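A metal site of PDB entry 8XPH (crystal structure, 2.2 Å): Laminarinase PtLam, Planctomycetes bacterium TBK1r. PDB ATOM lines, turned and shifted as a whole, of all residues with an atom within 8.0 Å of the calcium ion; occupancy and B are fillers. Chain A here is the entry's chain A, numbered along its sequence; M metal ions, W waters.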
ATOM      1  N   GLN A  12       6.105 -11.828  32.329  1.00  0.00           N
ATOM      2  CA  GLN A  12       6.020 -10.395  32.148  1.00  0.00           C
ATOM      3  C   GLN A  12       5.344 -10.116  30.809  1.00  0.00           C
ATOM      4  O   GLN A  12       5.875 -10.484  29.767  1.00  0.00           O
ATOM      5  CB  GLN A  12       7.427  -9.773  32.203  1.00  0.00           C
ATOM      6  CG  GLN A  12       7.976  -9.643  33.623  1.00  0.00           C
ATOM      7  CD  GLN A  12       7.276  -8.571  34.430  1.00  0.00           C
ATOM      8  OE1 GLN A  12       6.577  -8.858  35.408  1.00  0.00           O
ATOM      9  NE2 GLN A  12       7.452  -7.315  34.019  1.00  0.00           N
ATOM     10  N   GLU A  13       4.166  -9.495  30.858  1.00  0.00           N
ATOM     11  CA  GLU A  13       3.347  -9.273  29.673  1.00  0.00           C
ATOM     12  C   GLU A  13       3.600  -7.882  29.085  1.00  0.00           C
ATOM     13  O   GLU A  13       3.193  -7.622  27.955  1.00  0.00           O
ATOM     14  CB  GLU A  13       1.872  -9.480  30.005  1.00  0.00           C
ATOM     15  CG  GLU A  13       1.532 -10.907  30.431  1.00  0.00           C
ATOM     16  CD  GLU A  13       1.759 -11.967  29.371  1.00  0.00           C
ATOM     17  OE1 GLU A  13       1.491 -11.698  28.180  1.00  0.00           O
ATOM     18  OE2 GLU A  13       2.187 -13.091  29.732  1.00  0.00           O
ATOM     19  N   PHE A  14       4.258  -7.013  29.860  1.00  0.00           N
ATOM     20  CA  PHE A  14       4.695  -5.699  29.397  1.00  0.00           C
ATOM     21  C   PHE A  14       3.497  -4.863  28.959  1.00  0.00           C
ATOM     22  O   PHE A  14       3.504  -4.240  27.899  1.00  0.00           O
ATOM     23  CB  PHE A  14       5.719  -5.799  28.265  1.00  0.00           C
ATOM     24  CG  PHE A  14       6.984  -6.566  28.636  1.00  0.00           C
ATOM     25  CD1 PHE A  14       7.844  -6.098  29.620  1.00  0.00           C
ATOM     26  CD2 PHE A  14       7.314  -7.757  27.976  1.00  0.00           C
ATOM     27  CE1 PHE A  14       8.993  -6.790  29.946  1.00  0.00           C
ATOM     28  CE2 PHE A  14       8.466  -8.440  28.306  1.00  0.00           C
ATOM     29  CZ  PHE A  14       9.304  -7.966  29.287  1.00  0.00           C
ATOM     30  N   ASP A  15       2.492  -4.805  29.836  1.00  0.00           N
ATOM     31  CA  ASP A  15       1.211  -4.176  29.542  1.00  0.00           C
ATOM     32  C   ASP A  15       1.146  -2.750  30.062  1.00  0.00           C
ATOM     33  O   ASP A  15       0.291  -1.983  29.626  1.00  0.00           O
ATOM     34  CB  ASP A  15       0.075  -4.983  30.154  1.00  0.00           C
ATOM     35  CG  ASP A  15       0.075  -5.060  31.676  1.00  0.00           C
ATOM     36  OD1 ASP A  15       0.968  -5.737  32.246  1.00  0.00           O
ATOM     37  OD2 ASP A  15      -0.821  -4.434  32.296  1.00  0.00           O
ATOM     38  N   GLY A  16       2.021  -2.395  31.021  1.00  0.00           N
ATOM     39  CA  GLY A  16       1.902  -1.136  31.731  1.00  0.00           C
ATOM     40  C   GLY A  16       2.382   0.053  30.911  1.00  0.00           C
ATOM     41  O   GLY A  16       2.467  -0.015  29.674  1.00  0.00           O
ATOM     42  N   ARG A  51       4.996   0.151  25.595  1.00  0.00           N
ATOM     43  CA  ARG A  51       4.085   0.795  24.659  1.00  0.00           C
ATOM     44  C   ARG A  51       3.287  -0.281  23.944  1.00  0.00           C
ATOM     45  O   ARG A  51       3.877  -1.199  23.380  1.00  0.00           O
ATOM     46  CB  ARG A  51       4.948   1.593  23.666  1.00  0.00           C
ATOM     47  CG  ARG A  51       4.248   2.698  22.896  1.00  0.00           C
ATOM     48  CD  ARG A  51       5.257   3.737  22.397  1.00  0.00           C
ATOM     49  NE  ARG A  51       6.022   3.363  21.202  1.00  0.00           N
ATOM     50  CZ  ARG A  51       6.858   4.172  20.543  1.00  0.00           C
ATOM     51  NH1 ARG A  51       7.127   5.382  20.999  1.00  0.00           N
ATOM     52  NH2 ARG A  51       7.438   3.766  19.434  1.00  0.00           N
ATOM     53  N   ASP A  52       1.946  -0.173  23.983  1.00  0.00           N
ATOM     54  CA  ASP A  52       1.060  -0.969  23.140  1.00  0.00           C
ATOM     55  C   ASP A  52       1.196  -2.466  23.424  1.00  0.00           C
ATOM     56  O   ASP A  52       1.045  -3.281  22.512  1.00  0.00           O
ATOM     57  CB  ASP A  52       1.249  -0.629  21.663  1.00  0.00           C
ATOM     58  CG  ASP A  52       1.077   0.838  21.307  1.00  0.00           C
ATOM     59  OD1 ASP A  52       0.080   1.437  21.750  1.00  0.00           O
ATOM     60  OD2 ASP A  52       1.949   1.382  20.581  1.00  0.00           O
ATOM     61  N   GLY A  53       1.453  -2.820  24.692  1.00  0.00           N
ATOM     62  CA  GLY A  53       1.573  -4.210  25.100  1.00  0.00           C
ATOM     63  C   GLY A  53       2.941  -4.802  24.756  1.00  0.00           C
ATOM     64  O   GLY A  53       3.067  -6.020  24.636  1.00  0.00           O
ATOM     65  N   ASN A  54       3.951  -3.935  24.645  1.00  0.00           N
ATOM     66  CA  ASN A  54       5.296  -4.352  24.264  1.00  0.00           C
ATOM     67  C   ASN A  54       6.331  -3.699  25.167  1.00  0.00           C
ATOM     68  O   ASN A  54       6.184  -2.532  25.555  1.00  0.00           O
ATOM     69  CB  ASN A  54       5.625  -3.999  22.820  1.00  0.00           C
ATOM     70  CG  ASN A  54       4.883  -4.846  21.818  1.00  0.00           C
ATOM     71  OD1 ASN A  54       4.095  -4.317  21.020  1.00  0.00           O
ATOM     72  ND2 ASN A  54       5.127  -6.135  21.813  1.00  0.00           N
ATOM     73  N   LEU A  55       7.374  -4.462  25.503  1.00  0.00           N
ATOM     74  CA  LEU A  55       8.649  -3.879  25.901  1.00  0.00           C
ATOM     75  C   LEU A  55       9.383  -3.489  24.628  1.00  0.00           C
ATOM     76  O   LEU A  55       9.489  -4.290  23.692  1.00  0.00           O
ATOM     77  CB  LEU A  55       9.487  -4.843  26.742  1.00  0.00           C
ATOM     78  CG  LEU A  55      10.981  -4.518  26.861  1.00  0.00           C
ATOM     79  CD1 LEU A  55      11.234  -3.334  27.790  1.00  0.00           C
ATOM     80  CD2 LEU A  55      11.777  -5.726  27.302  1.00  0.00           C
ATOM     81  N   ARG A  90       8.165 -13.836  22.944  1.00  0.00           N
ATOM     82  CA  ARG A  90       7.711 -13.394  21.638  1.00  0.00           C
ATOM     83  C   ARG A  90       8.407 -12.071  21.321  1.00  0.00           C
ATOM     84  O   ARG A  90       8.097 -11.045  21.943  1.00  0.00           O
ATOM     85  CB  ARG A  90       6.181 -13.280  21.646  1.00  0.00           C
ATOM     86  CG  ARG A  90       5.586 -13.047  20.273  1.00  0.00           C
ATOM     87  CD  ARG A  90       4.077 -13.078  20.274  1.00  0.00           C
ATOM     88  NE  ARG A  90       3.532 -12.972  18.918  1.00  0.00           N
ATOM     89  CZ  ARG A  90       3.021 -11.876  18.373  1.00  0.00           C
ATOM     90  NH1 ARG A  90       3.036 -10.720  19.029  1.00  0.00           N
ATOM     91  NH2 ARG A  90       2.531 -11.922  17.147  1.00  0.00           N
ATOM     92  N   VAL A 244       9.429  -6.786  22.545  1.00  0.00           N
ATOM     93  CA  VAL A 244       9.131  -7.989  23.315  1.00  0.00           C
ATOM     94  C   VAL A 244       7.682  -7.921  23.769  1.00  0.00           C
ATOM     95  O   VAL A 244       7.333  -7.084  24.600  1.00  0.00           O
ATOM     96  CB  VAL A 244      10.086  -8.158  24.519  1.00  0.00           C
ATOM     97  CG1 VAL A 244       9.887  -9.510  25.201  1.00  0.00           C
ATOM     98  CG2 VAL A 244      11.543  -7.972  24.137  1.00  0.00           C
ATOM     99  N   ASP A 245       6.837  -8.819  23.232  1.00  0.00           N
ATOM    100  CA  ASP A 245       5.429  -8.844  23.572  1.00  0.00           C
ATOM    101  C   ASP A 245       5.252  -9.431  24.975  1.00  0.00           C
ATOM    102  O   ASP A 245       4.447  -8.938  25.769  1.00  0.00           O
ATOM    103  CB  ASP A 245       4.618  -9.610  22.538  1.00  0.00           C
ATOM    104  CG  ASP A 245       3.103  -9.551  22.698  1.00  0.00           C
ATOM    105  OD1 ASP A 245       2.615  -8.714  23.490  1.00  0.00           O
ATOM    106  OD2 ASP A 245       2.407 -10.367  22.052  1.00  0.00           O
ATOM    107  N   TRP A 246       6.006 -10.503  25.264  1.00  0.00           N
ATOM    108  CA  TRP A 246       5.953 -11.141  26.571  1.00  0.00           C
ATOM    109  C   TRP A 246       7.109 -12.124  26.746  1.00  0.00           C
ATOM    110  O   TRP A 246       7.758 -12.516  25.783  1.00  0.00           O
ATOM    111  CB  TRP A 246       4.597 -11.826  26.779  1.00  0.00           C
ATOM    112  CG  TRP A 246       4.109 -12.657  25.617  1.00  0.00           C
ATOM    113  CD1 TRP A 246       3.175 -12.290  24.695  1.00  0.00           C
ATOM    114  CD2 TRP A 246       4.493 -14.003  25.280  1.00  0.00           C
ATOM    115  NE1 TRP A 246       2.957 -13.311  23.809  1.00  0.00           N
ATOM    116  CE2 TRP A 246       3.746 -14.373  24.138  1.00  0.00           C
ATOM    117  CE3 TRP A 246       5.393 -14.932  25.821  1.00  0.00           C
ATOM    118  CZ2 TRP A 246       3.882 -15.628  23.540  1.00  0.00           C
ATOM    119  CZ3 TRP A 246       5.530 -16.164  25.222  1.00  0.00           C
ATOM    120  CH2 TRP A 246       4.779 -16.507  24.094  1.00  0.00           C
ATOM    121  N   ILE A 247       7.358 -12.468  28.021  1.00  0.00           N
ATOM    122  CA  ILE A 247       8.216 -13.566  28.404  1.00  0.00           C
ATOM    123  C   ILE A 247       7.424 -14.445  29.372  1.00  0.00           C
ATOM    124  O   ILE A 247       6.871 -13.936  30.350  1.00  0.00           O
ATOM    125  CB  ILE A 247       9.514 -13.080  29.081  1.00  0.00           C
ATOM    126  CG1 ILE A 247      10.111 -11.838  28.446  1.00  0.00           C
ATOM    127  CG2 ILE A 247      10.553 -14.208  29.155  1.00  0.00           C
ATOM    128  CD1 ILE A 247      11.052 -11.085  29.367  1.00  0.00           C
ATOM    129  N   ARG A 248       7.357 -15.749  29.098  1.00  0.00           N
ATOM    130  CA  ARG A 248       6.529 -16.649  29.894  1.00  0.00           C
ATOM    131  C   ARG A 248       7.320 -17.882  30.291  1.00  0.00           C
ATOM    132  O   ARG A 248       8.050 -18.440  29.477  1.00  0.00           O
ATOM    133  CB  ARG A 248       5.266 -17.044  29.113  1.00  0.00           C
ATOM    134  CG  ARG A 248       4.283 -15.909  28.888  1.00  0.00           C
ATOM    135  CD  ARG A 248       3.155 -16.295  27.967  1.00  0.00           C
ATOM    136  NE  ARG A 248       2.296 -15.143  27.667  1.00  0.00           N
ATOM    137  CZ  ARG A 248       1.398 -15.090  26.689  1.00  0.00           C
ATOM    138  NH1 ARG A 248       1.224 -16.118  25.879  1.00  0.00           N
ATOM    139  NH2 ARG A 248       0.672 -13.995  26.518  1.00  0.00           N
HETATM  140 CA    CA M   1       2.122  -7.940  25.881  1.00  0.00          CA
HETATM  141  O   HOH W   1       1.253 -10.116  26.191  1.00  0.00           O
HETATM  142  O   HOH W   2       0.727  -6.793  27.320  1.00  0.00           O
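The side-chain carboxylate (OD2) of Asp 245 sits close to the indole nitrogen (NE1) of Trp 246 (3.5 Å). The guanidinium group of Arg 248 is in salt-bridge range of the side-chain carboxylate of Glu 13, at 2.9 Å. NH1 of Arg 90 is in salt-bridge range of OD2 of Asp 245, at 3.1 Å. The backbone NH (N) of Asp 245 sits close to the side-chain amide nitrogen (ND2) of Asn 54, 3.5 Å away.
Three residues have an atom within 4 Å of the calcium ion: Glu 13, Gly 53 and Asp 245. Along chain A the residues within 4 Å of the calcium ion span positions 13 to 245.
The calcium ion is bound by water W2 (2.3 Å), the backbone carbonyl oxygen of Glu 13 (2.4 Å), water W1 (2.4 Å), the backbone carbonyl oxygen of Gly 53 (2.5 Å), the backbone carbonyl oxygen of Asp 245 (2.5 Å) and the side-chain carboxylate of Asp 245 (2.6 Å). The calcium ion has six donor atoms within binding distance.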
